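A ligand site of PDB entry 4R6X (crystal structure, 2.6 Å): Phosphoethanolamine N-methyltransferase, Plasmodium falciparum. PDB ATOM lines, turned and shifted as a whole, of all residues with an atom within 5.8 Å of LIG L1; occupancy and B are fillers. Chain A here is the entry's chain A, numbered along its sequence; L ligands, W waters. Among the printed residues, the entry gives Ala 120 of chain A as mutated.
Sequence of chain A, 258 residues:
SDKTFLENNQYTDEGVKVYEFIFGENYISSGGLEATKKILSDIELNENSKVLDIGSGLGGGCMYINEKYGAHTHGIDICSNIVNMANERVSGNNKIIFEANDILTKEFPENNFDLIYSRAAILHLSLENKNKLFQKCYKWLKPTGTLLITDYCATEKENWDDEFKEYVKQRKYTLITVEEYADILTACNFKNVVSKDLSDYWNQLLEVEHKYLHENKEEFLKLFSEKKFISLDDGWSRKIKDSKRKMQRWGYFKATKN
O5 of LIG L1 sits at hydrogen-bond distance from OD1 of Asp 77, at 2.4 Å.
OG of Ser 29 is in hydrogen-bond range of O1 of LIG L1, at 2.4 Å.
O of Gly 55 lies within hydrogen-bond range of N1 of LIG L1, 2.5 Å away.
OD1 of Asp 102 lies within hydrogen-bond range of N4 of LIG L1, 2.8 Å away.
O2 of LIG L1 lies within hydrogen-bond range of N of Ile 28, 3.0 Å away.
N of Ile 103 is in hydrogen-bond range of N5 of LIG L1.
A nitrogen (N6) of LIG L1 is in hydrogen-bond range of the backbone NH (N) of Ile 78 (3.2 Å).
The backbone carbonyl oxygen (O) of Arg 119 sits at hydrogen-bond distance from a nitrogen (N1) of LIG L1 (3.3 Å).
The side-chain hydroxyl (OH) of Tyr 11 lies close to a sulfur (S1) of LIG L1 (3.6 Å).
SG of Cys 79 sits at hydrogen-bond distance from O5 of LIG L1 (3.6 Å).
O of Ile 28 lies close to N1 of LG2 L2, at 3.3 Å.
The side-chain carboxylate (OD1) of Asp 77 sits at hydrogen-bond distance from the backbone NH (N) of Cys 79.
The backbone carbonyl oxygen (O) of Asp 77 sits at hydrogen-bond distance from the backbone NH (N) of Asn 101, 2.9 Å away.
The side-chain carboxylate of Asp 77 is in hydrogen-bond range of the backbone NH of Gly 57 (3.0 Å).
The backbone NH of Gly 55 is in hydrogen-bond range of the backbone carbonyl oxygen of Ile 76.
The backbone carbonyl oxygen (O) of Asn 101 sits close to the backbone NH (N) of Ile 78 (3.4 Å).
The side-chain hydroxyl of Tyr 11 is in hydrogen-bond range of a ring nitrogen (NE2) of His 124.
The backbone carbonyl oxygen (O) of Leu 6 lies within hydrogen-bond range of the backbone NH (N) of Tyr 11, at 2.8 Å.
OH of Tyr 27 lies within hydrogen-bond range of O of Gly 60, 3.0 Å away.
The backbone carbonyl oxygen (O) of Ala 120 lies close to a sulfur (S1) of LIG L1 (3.7 Å).
Residues that only touch LIG L1: Ala 121, Ser 56, Ile 82, His 124, Tyr 27, Asn 101, Leu 6, Gly 57 and Leu 125.
The nearest printed residue that does not touch LIG L1 is Ile 76 (4.01 Å).
Water W1 lies within hydrogen-bond range of N of Leu 58, O2 of LIG L1, O of Asn 26 and O of Ser 56.
Water W2 bridges a nitrogen (N1) of LIG L1 (3.1 Å) and the side-chain carboxylate (OD2) of Asp 53 (3.3 Å).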
ATOM      1  N   LEU A   6       3.461  17.596  12.512  1.00  0.00           N
ATOM      2  CA  LEU A   6       2.512  16.982  11.595  1.00  0.00           C
ATOM      3  C   LEU A   6       2.970  15.609  11.120  1.00  0.00           C
ATOM      4  O   LEU A   6       2.178  14.664  11.050  1.00  0.00           O
ATOM      5  CB  LEU A   6       2.228  17.901  10.414  1.00  0.00           C
ATOM      6  CG  LEU A   6       1.504  19.207  10.737  1.00  0.00           C
ATOM      7  CD1 LEU A   6       1.363  20.081   9.498  1.00  0.00           C
ATOM      8  CD2 LEU A   6       0.143  18.929  11.350  1.00  0.00           C
ATOM      9  N   TYR A  11      -0.081  13.109  10.762  1.00  0.00           N
ATOM     10  CA  TYR A  11       0.228  12.673   9.406  1.00  0.00           C
ATOM     11  C   TYR A  11       1.470  11.782   9.325  1.00  0.00           C
ATOM     12  O   TYR A  11       2.380  12.052   8.544  1.00  0.00           O
ATOM     13  CB  TYR A  11       0.367  13.869   8.463  1.00  0.00           C
ATOM     14  CG  TYR A  11      -0.860  14.740   8.418  1.00  0.00           C
ATOM     15  CD1 TYR A  11      -2.054  14.258   7.894  1.00  0.00           C
ATOM     16  CD2 TYR A  11      -0.842  16.046   8.897  1.00  0.00           C
ATOM     17  CE1 TYR A  11      -3.186  15.043   7.854  1.00  0.00           C
ATOM     18  CE2 TYR A  11      -1.967  16.837   8.857  1.00  0.00           C
ATOM     19  CZ  TYR A  11      -3.141  16.331   8.329  1.00  0.00           C
ATOM     20  OH  TYR A  11      -4.266  17.122   8.289  1.00  0.00           O
ATOM     21  N   ASN A  26      -6.187   8.267  -2.529  1.00  0.00           N
ATOM     22  CA  ASN A  26      -5.468   9.524  -2.818  1.00  0.00           C
ATOM     23  C   ASN A  26      -6.025  10.770  -2.126  1.00  0.00           C
ATOM     24  O   ASN A  26      -5.738  11.895  -2.553  1.00  0.00           O
ATOM     25  CB  ASN A  26      -5.336   9.765  -4.332  1.00  0.00           C
ATOM     26  CG  ASN A  26      -4.860   8.530  -5.077  1.00  0.00           C
ATOM     27  OD1 ASN A  26      -3.952   7.836  -4.644  1.00  0.00           O
ATOM     28  ND2 ASN A  26      -5.496   8.259  -6.215  1.00  0.00           N
ATOM     29  N   TYR A  27      -6.798  10.599  -1.055  1.00  0.00           N
ATOM     30  CA  TYR A  27      -7.370  11.749  -0.347  1.00  0.00           C
ATOM     31  C   TYR A  27      -7.178  11.713   1.164  1.00  0.00           C
ATOM     32  O   TYR A  27      -7.071  10.637   1.758  1.00  0.00           O
ATOM     33  CB  TYR A  27      -8.864  11.894  -0.669  1.00  0.00           C
ATOM     34  CG  TYR A  27      -9.132  12.446  -2.053  1.00  0.00           C
ATOM     35  CD1 TYR A  27      -9.023  13.805  -2.306  1.00  0.00           C
ATOM     36  CD2 TYR A  27      -9.500  11.616  -3.094  1.00  0.00           C
ATOM     37  CE1 TYR A  27      -9.264  14.324  -3.565  1.00  0.00           C
ATOM     38  CE2 TYR A  27      -9.752  12.116  -4.359  1.00  0.00           C
ATOM     39  CZ  TYR A  27      -9.628  13.469  -4.585  1.00  0.00           C
ATOM     40  OH  TYR A  27      -9.875  13.978  -5.836  1.00  0.00           O
ATOM     41  N   ILE A  28      -7.126  12.896   1.782  1.00  0.00           N
ATOM     42  CA  ILE A  28      -7.048  13.010   3.231  1.00  0.00           C
ATOM     43  C   ILE A  28      -8.095  14.006   3.758  1.00  0.00           C
ATOM     44  O   ILE A  28      -7.946  14.558   4.845  1.00  0.00           O
ATOM     45  CB  ILE A  28      -5.639  13.435   3.719  1.00  0.00           C
ATOM     46  CG1 ILE A  28      -4.548  12.953   2.746  1.00  0.00           C
ATOM     47  CG2 ILE A  28      -5.359  12.899   5.118  1.00  0.00           C
ATOM     48  CD1 ILE A  28      -3.148  13.298   3.188  1.00  0.00           C
ATOM     49  N   SER A  29      -9.155  14.223   2.983  1.00  0.00           N
ATOM     50  CA  SER A  29     -10.237  15.117   3.395  1.00  0.00           C
ATOM     51  C   SER A  29     -11.611  14.554   3.006  1.00  0.00           C
ATOM     52  O   SER A  29     -11.703  13.678   2.142  1.00  0.00           O
ATOM     53  CB  SER A  29     -10.045  16.522   2.826  1.00  0.00           C
ATOM     54  OG  SER A  29     -10.021  16.500   1.413  1.00  0.00           O
ATOM     55  N   ASP A  53      -1.967  23.905  -5.480  1.00  0.00           N
ATOM     56  CA  ASP A  53      -2.689  23.130  -4.478  1.00  0.00           C
ATOM     57  C   ASP A  53      -1.966  23.205  -3.136  1.00  0.00           C
ATOM     58  O   ASP A  53      -1.048  22.435  -2.864  1.00  0.00           O
ATOM     59  CB  ASP A  53      -2.849  21.676  -4.919  1.00  0.00           C
ATOM     60  CG  ASP A  53      -3.823  20.897  -4.057  1.00  0.00           C
ATOM     61  OD1 ASP A  53      -4.276  21.422  -3.017  1.00  0.00           O
ATOM     62  OD2 ASP A  53      -4.154  19.745  -4.418  1.00  0.00           O
ATOM     63  N   ILE A  54      -2.410  24.128  -2.280  1.00  0.00           N
ATOM     64  CA  ILE A  54      -1.821  24.291  -0.953  1.00  0.00           C
ATOM     65  C   ILE A  54      -2.306  23.179  -0.029  1.00  0.00           C
ATOM     66  O   ILE A  54      -3.496  23.063   0.252  1.00  0.00           O
ATOM     67  CB  ILE A  54      -2.190  25.665  -0.343  1.00  0.00           C
ATOM     68  CG1 ILE A  54      -1.758  26.797  -1.278  1.00  0.00           C
ATOM     69  CG2 ILE A  54      -1.551  25.809   1.030  1.00  0.00           C
ATOM     70  CD1 ILE A  54      -2.109  28.175  -0.761  1.00  0.00           C
ATOM     71  N   GLY A  55      -1.370  22.364   0.443  1.00  0.00           N
ATOM     72  CA  GLY A  55      -1.711  21.186   1.210  1.00  0.00           C
ATOM     73  C   GLY A  55      -2.280  20.126   0.298  1.00  0.00           C
ATOM     74  O   GLY A  55      -3.422  19.690   0.457  1.00  0.00           O
ATOM     75  N   SER A  56      -1.483  19.709  -0.682  1.00  0.00           N
ATOM     76  CA  SER A  56      -1.930  18.764  -1.698  1.00  0.00           C
ATOM     77  C   SER A  56      -2.154  17.356  -1.166  1.00  0.00           C
ATOM     78  O   SER A  56      -3.013  16.627  -1.663  1.00  0.00           O
ATOM     79  CB  SER A  56      -0.936  18.734  -2.872  1.00  0.00           C
ATOM     80  OG  SER A  56       0.387  18.548  -2.421  1.00  0.00           O
ATOM     81  N   GLY A  57      -1.398  16.975  -0.138  1.00  0.00           N
ATOM     82  CA  GLY A  57      -1.572  15.669   0.483  1.00  0.00           C
ATOM     83  C   GLY A  57      -1.127  14.524  -0.416  1.00  0.00           C
ATOM     84  O   GLY A  57       0.008  14.507  -0.899  1.00  0.00           O
ATOM     85  N   LEU A  58      -2.021  13.563  -0.635  1.00  0.00           N
ATOM     86  CA  LEU A  58      -1.715  12.410  -1.479  1.00  0.00           C
ATOM     87  C   LEU A  58      -1.880  12.730  -2.960  1.00  0.00           C
ATOM     88  O   LEU A  58      -1.645  11.875  -3.809  1.00  0.00           O
ATOM     89  CB  LEU A  58      -2.561  11.201  -1.068  1.00  0.00           C
ATOM     90  CG  LEU A  58      -2.186  10.552   0.267  1.00  0.00           C
ATOM     91  CD1 LEU A  58      -3.131   9.413   0.600  1.00  0.00           C
ATOM     92  CD2 LEU A  58      -0.739  10.058   0.232  1.00  0.00           C
ATOM     93  N   GLY A  60      -4.625  13.651  -4.692  1.00  0.00           N
ATOM     94  CA  GLY A  60      -5.899  13.347  -5.319  1.00  0.00           C
ATOM     95  C   GLY A  60      -6.541  14.542  -6.002  1.00  0.00           C
ATOM     96  O   GLY A  60      -7.182  14.409  -7.043  1.00  0.00           O
ATOM     97  N   GLY A  61      -6.365  15.716  -5.409  1.00  0.00           N
ATOM     98  CA  GLY A  61      -6.879  16.948  -5.985  1.00  0.00           C
ATOM     99  C   GLY A  61      -6.174  17.312  -7.279  1.00  0.00           C
ATOM    100  O   GLY A  61      -6.825  17.651  -8.263  1.00  0.00           O
ATOM    101  N   ILE A  76       1.823  21.820  -3.122  1.00  0.00           N
ATOM    102  CA  ILE A  76       2.731  22.061  -2.011  1.00  0.00           C
ATOM    103  C   ILE A  76       2.195  21.437  -0.732  1.00  0.00           C
ATOM    104  O   ILE A  76       1.040  21.668  -0.350  1.00  0.00           O
ATOM    105  CB  ILE A  76       2.937  23.577  -1.780  1.00  0.00           C
ATOM    106  CG1 ILE A  76       3.473  24.247  -3.039  1.00  0.00           C
ATOM    107  CG2 ILE A  76       3.882  23.813  -0.615  1.00  0.00           C
ATOM    108  CD1 ILE A  76       4.918  23.903  -3.367  1.00  0.00           C
ATOM    109  N   ASP A  77       3.024  20.637  -0.067  1.00  0.00           N
ATOM    110  CA  ASP A  77       2.671  20.056   1.228  1.00  0.00           C
ATOM    111  C   ASP A  77       3.878  20.069   2.159  1.00  0.00           C
ATOM    112  O   ASP A  77       4.988  19.756   1.730  1.00  0.00           O
ATOM    113  CB  ASP A  77       2.145  18.644   1.049  1.00  0.00           C
ATOM    114  CG  ASP A  77       1.392  18.139   2.269  1.00  0.00           C
ATOM    115  OD1 ASP A  77       2.039  17.831   3.292  1.00  0.00           O
ATOM    116  OD2 ASP A  77       0.144  18.056   2.208  1.00  0.00           O
ATOM    117  N   ILE A  78       3.662  20.432   3.413  1.00  0.00           N
ATOM    118  CA  ILE A  78       4.771  20.583   4.363  1.00  0.00           C
ATOM    119  C   ILE A  78       5.361  19.253   4.830  1.00  0.00           C
ATOM    120  O   ILE A  78       6.507  19.194   5.260  1.00  0.00           O
ATOM    121  CB  ILE A  78       4.346  21.454   5.585  1.00  0.00           C
ATOM    122  CG1 ILE A  78       5.583  21.968   6.337  1.00  0.00           C
ATOM    123  CG2 ILE A  78       3.417  20.676   6.503  1.00  0.00           C
ATOM    124  CD1 ILE A  78       5.248  22.877   7.507  1.00  0.00           C
ATOM    125  N   CYS A  79       4.585  18.178   4.732  1.00  0.00           N
ATOM    126  CA  CYS A  79       5.048  16.868   5.162  1.00  0.00           C
ATOM    127  C   CYS A  79       5.785  16.123   4.040  1.00  0.00           C
ATOM    128  O   CYS A  79       5.198  15.810   3.005  1.00  0.00           O
ATOM    129  CB  CYS A  79       3.881  16.018   5.683  1.00  0.00           C
ATOM    130  SG  CYS A  79       3.103  16.656   7.173  1.00  0.00           S
ATOM    131  N   ILE A  82       4.512  12.467   3.140  1.00  0.00           N
ATOM    132  CA  ILE A  82       3.274  12.440   2.370  1.00  0.00           C
ATOM    133  C   ILE A  82       3.550  12.705   0.896  1.00  0.00           C
ATOM    134  O   ILE A  82       2.991  12.047   0.015  1.00  0.00           O
ATOM    135  CB  ILE A  82       2.251  13.471   2.895  1.00  0.00           C
ATOM    136  CG1 ILE A  82       1.928  13.203   4.357  1.00  0.00           C
ATOM    137  CG2 ILE A  82       0.974  13.436   2.063  1.00  0.00           C
ATOM    138  CD1 ILE A  82       0.832  14.097   4.908  1.00  0.00           C
ATOM    139  N   ASN A 101       7.274  21.407   1.073  1.00  0.00           N
ATOM    140  CA  ASN A 101       7.659  22.737   1.523  1.00  0.00           C
ATOM    141  C   ASN A 101       6.573  23.407   2.354  1.00  0.00           C
ATOM    142  O   ASN A 101       5.381  23.140   2.173  1.00  0.00           O
ATOM    143  CB  ASN A 101       7.996  23.619   0.310  1.00  0.00           C
ATOM    144  CG  ASN A 101       9.254  24.430   0.514  1.00  0.00           C
ATOM    145  OD1 ASN A 101       9.513  24.939   1.609  1.00  0.00           O
ATOM    146  ND2 ASN A 101      10.060  24.540  -0.537  1.00  0.00           N
ATOM    147  N   ASP A 102       6.980  24.286   3.261  1.00  0.00           N
ATOM    148  CA  ASP A 102       6.028  25.121   3.995  1.00  0.00           C
ATOM    149  C   ASP A 102       5.512  26.190   3.043  1.00  0.00           C
ATOM    150  O   ASP A 102       6.294  26.866   2.376  1.00  0.00           O
ATOM    151  CB  ASP A 102       6.700  25.774   5.204  1.00  0.00           C
ATOM    152  CG  ASP A 102       5.708  26.408   6.164  1.00  0.00           C
ATOM    153  OD1 ASP A 102       4.531  26.595   5.788  1.00  0.00           O
ATOM    154  OD2 ASP A 102       6.105  26.705   7.308  1.00  0.00           O
ATOM    155  N   ILE A 103       4.189  26.332   2.967  1.00  0.00           N
ATOM    156  CA  ILE A 103       3.584  27.284   2.053  1.00  0.00           C
ATOM    157  C   ILE A 103       3.846  28.723   2.493  1.00  0.00           C
ATOM    158  O   ILE A 103       3.846  29.641   1.677  1.00  0.00           O
ATOM    159  CB  ILE A 103       2.054  27.034   1.900  1.00  0.00           C
ATOM    160  CG1 ILE A 103       1.481  27.832   0.729  1.00  0.00           C
ATOM    161  CG2 ILE A 103       1.323  27.363   3.207  1.00  0.00           C
ATOM    162  CD1 ILE A 103       2.012  27.390  -0.621  1.00  0.00           C
ATOM    163  N   LEU A 104       4.102  28.906   3.781  1.00  0.00           N
ATOM    164  CA  LEU A 104       4.342  30.229   4.345  1.00  0.00           C
ATOM    165  C   LEU A 104       5.714  30.788   3.967  1.00  0.00           C
ATOM    166  O   LEU A 104       5.937  31.999   4.034  1.00  0.00           O
ATOM    167  CB  LEU A 104       4.185  30.195   5.868  1.00  0.00           C
ATOM    168  CG  LEU A 104       2.803  29.809   6.393  1.00  0.00           C
ATOM    169  CD1 LEU A 104       2.837  29.602   7.891  1.00  0.00           C
ATOM    170  CD2 LEU A 104       1.781  30.880   6.024  1.00  0.00           C
ATOM    171  N   SER A 118      -7.123  24.902  -2.169  1.00  0.00           N
ATOM    172  CA  SER A 118      -6.739  24.313  -0.889  1.00  0.00           C
ATOM    173  C   SER A 118      -7.911  23.640  -0.175  1.00  0.00           C
ATOM    174  O   SER A 118      -8.964  24.252  -0.010  1.00  0.00           O
ATOM    175  CB  SER A 118      -6.091  25.356   0.017  1.00  0.00           C
ATOM    176  OG  SER A 118      -5.575  24.759   1.192  1.00  0.00           O
ATOM    177  N   ARG A 119      -7.706  22.398   0.240  1.00  0.00           N
ATOM    178  CA  ARG A 119      -8.744  21.639   0.925  1.00  0.00           C
ATOM    179  C   ARG A 119      -8.234  21.126   2.275  1.00  0.00           C
ATOM    180  O   ARG A 119      -7.282  20.357   2.324  1.00  0.00           O
ATOM    181  CB  ARG A 119      -9.162  20.430   0.076  1.00  0.00           C
ATOM    182  CG  ARG A 119      -9.516  20.742  -1.370  1.00  0.00           C
ATOM    183  CD  ARG A 119     -10.964  21.162  -1.514  1.00  0.00           C
ATOM    184  NE  ARG A 119     -11.865  20.260  -0.793  1.00  0.00           N
ATOM    185  CZ  ARG A 119     -12.358  19.135  -1.292  1.00  0.00           C
ATOM    186  NH1 ARG A 119     -12.041  18.755  -2.524  1.00  0.00           N
ATOM    187  NH2 ARG A 119     -13.154  18.373  -0.559  1.00  0.00           N
ATOM    188  N   ALA A 120      -8.887  21.577   3.345  1.00  0.00           N
ATOM    189  CA  ALA A 120      -8.603  21.091   4.697  1.00  0.00           C
ATOM    190  C   ALA A 120      -7.124  21.166   5.089  1.00  0.00           C
ATOM    191  O   ALA A 120      -6.575  20.202   5.618  1.00  0.00           O
ATOM    192  CB  ALA A 120      -9.127  19.666   4.872  1.00  0.00           C
ATOM    193  N   ALA A 121      -6.497  22.309   4.829  1.00  0.00           N
ATOM    194  CA  ALA A 121      -5.073  22.468   5.092  1.00  0.00           C
ATOM    195  C   ALA A 121      -4.762  23.700   5.946  1.00  0.00           C
ATOM    196  O   ALA A 121      -3.930  23.655   6.857  1.00  0.00           O
ATOM    197  CB  ALA A 121      -4.304  22.528   3.782  1.00  0.00           C
ATOM    198  N   ILE A 122      -5.448  24.792   5.645  1.00  0.00           N
ATOM    199  CA  ILE A 122      -5.190  26.082   6.279  1.00  0.00           C
ATOM    200  C   ILE A 122      -5.558  26.092   7.776  1.00  0.00           C
ATOM    201  O   ILE A 122      -5.076  26.925   8.541  1.00  0.00           O
ATOM    202  CB  ILE A 122      -5.897  27.226   5.500  1.00  0.00           C
ATOM    203  CG1 ILE A 122      -5.415  27.214   4.040  1.00  0.00           C
ATOM    204  CG2 ILE A 122      -5.653  28.585   6.124  1.00  0.00           C
ATOM    205  CD1 ILE A 122      -6.044  28.284   3.185  1.00  0.00           C
ATOM    206  N   LEU A 123      -6.387  25.136   8.183  1.00  0.00           N
ATOM    207  CA  LEU A 123      -6.764  24.991   9.591  1.00  0.00           C
ATOM    208  C   LEU A 123      -5.558  24.735  10.502  1.00  0.00           C
ATOM    209  O   LEU A 123      -5.631  24.955  11.712  1.00  0.00           O
ATOM    210  CB  LEU A 123      -7.796  23.882   9.769  1.00  0.00           C
ATOM    211  CG  LEU A 123      -7.252  22.451   9.820  1.00  0.00           C
ATOM    212  CD1 LEU A 123      -8.316  21.518  10.355  1.00  0.00           C
ATOM    213  CD2 LEU A 123      -6.786  21.980   8.451  1.00  0.00           C
ATOM    214  N   HIS A 124      -4.471  24.258   9.915  1.00  0.00           N
ATOM    215  CA  HIS A 124      -3.243  24.010  10.666  1.00  0.00           C
ATOM    216  C   HIS A 124      -2.483  25.309  10.937  1.00  0.00           C
ATOM    217  O   HIS A 124      -1.593  25.362  11.776  1.00  0.00           O
ATOM    218  CB  HIS A 124      -2.328  23.049   9.896  1.00  0.00           C
ATOM    219  CG  HIS A 124      -2.881  21.667   9.748  1.00  0.00           C
ATOM    220  ND1 HIS A 124      -2.949  20.772  10.796  1.00  0.00           N
ATOM    221  CD2 HIS A 124      -3.384  21.010   8.673  1.00  0.00           C
ATOM    222  CE1 HIS A 124      -3.478  19.635  10.380  1.00  0.00           C
ATOM    223  NE2 HIS A 124      -3.746  19.757   9.085  1.00  0.00           N
ATOM    224  N   LEU A 125      -2.855  26.364  10.211  1.00  0.00           N
ATOM    225  CA  LEU A 125      -2.188  27.654  10.334  1.00  0.00           C
ATOM    226  C   LEU A 125      -2.817  28.507  11.431  1.00  0.00           C
ATOM    227  O   LEU A 125      -4.027  28.491  11.626  1.00  0.00           O
ATOM    228  CB  LEU A 125      -2.227  28.410   9.004  1.00  0.00           C
ATOM    229  CG  LEU A 125      -1.124  28.146   7.967  1.00  0.00           C
ATOM    230  CD1 LEU A 125      -1.037  26.664   7.597  1.00  0.00           C
ATOM    231  CD2 LEU A 125      -1.355  28.988   6.726  1.00  0.00           C
HETATM  232  N1  LIG L   1      -5.625  18.626   0.059  1.00  0.00           N
HETATM  233  C1  LIG L   1      -5.491  17.214   0.484  1.00  0.00           C
HETATM  234  C2  LIG L   1      -4.753  17.117   1.881  1.00  0.00           C
HETATM  235  C3  LIG L   1      -5.630  17.313   3.132  1.00  0.00           C
HETATM  236  S1  LIG L   1      -4.849  17.070   4.757  1.00  0.00           S
HETATM  237  C4  LIG L   1      -6.806  16.556   0.420  1.00  0.00           C
HETATM  238  O1  LIG L   1      -7.818  17.205   0.648  1.00  0.00           O
HETATM  239  O2  LIG L   1      -6.890  15.389   0.133  1.00  0.00           O
HETATM  240  C5  LIG L   1      -3.902  18.550   5.196  1.00  0.00           C
HETATM  241  C6  LIG L   1      -2.666  18.799   4.534  1.00  0.00           C
HETATM  242  O3  LIG L   1      -2.303  20.183   4.767  1.00  0.00           O
HETATM  243  C7  LIG L   1      -1.612  17.990   5.193  1.00  0.00           C
HETATM  244  O4  LIG L   1      -1.101  17.036   4.294  1.00  0.00           O
HETATM  245  C8  LIG L   1      -0.567  18.932   5.590  1.00  0.00           C
HETATM  246  O5  LIG L   1       0.693  18.494   5.167  1.00  0.00           O
HETATM  247  C9  LIG L   1      -0.914  20.196   4.872  1.00  0.00           C
HETATM  248  N2  LIG L   1      -0.290  21.394   5.539  1.00  0.00           N
HETATM  249  C10 LIG L   1      -0.441  21.819   6.804  1.00  0.00           C
HETATM  250  N3  LIG L   1       0.305  22.926   6.948  1.00  0.00           N
HETATM  251  C11 LIG L   1       0.917  23.198   5.784  1.00  0.00           C
HETATM  252  C12 LIG L   1       1.790  24.212   5.368  1.00  0.00           C
HETATM  253  N4  LIG L   1       2.182  25.195   6.235  1.00  0.00           N
HETATM  254  N5  LIG L   1       2.243  24.198   4.095  1.00  0.00           N
HETATM  255  C13 LIG L   1       1.863  23.248   3.240  1.00  0.00           C
HETATM  256  N6  LIG L   1       1.015  22.255   3.613  1.00  0.00           N
HETATM  257  C14 LIG L   1       0.533  22.211   4.868  1.00  0.00           C
HETATM  258  C1  LG2 L   2      -8.987  15.029   9.157  1.00  0.00           C
HETATM  259  C2  LG2 L   2      -8.143  15.474   8.010  1.00  0.00           C
HETATM  260  O1  LG2 L   2      -9.466  13.809  11.990  1.00  0.00           O
HETATM  261  O2  LG2 L   2     -11.040  15.498  11.186  1.00  0.00           O
HETATM  262  O3  LG2 L   2      -9.243  16.156  12.791  1.00  0.00           O
HETATM  263  O4  LG2 L   2      -8.693  15.558  10.398  1.00  0.00           O
HETATM  264  N1  LG2 L   2      -8.553  16.670   7.312  1.00  0.00           N
HETATM  265  P1  LG2 L   2      -9.605  15.269  11.621  1.00  0.00           P
HETATM  266  O   HOH W   1      -4.538  13.920  -0.597  1.00  0.00           O
HETATM  267  O   HOH W   2      -6.620  18.234  -2.898  1.00  0.00           O
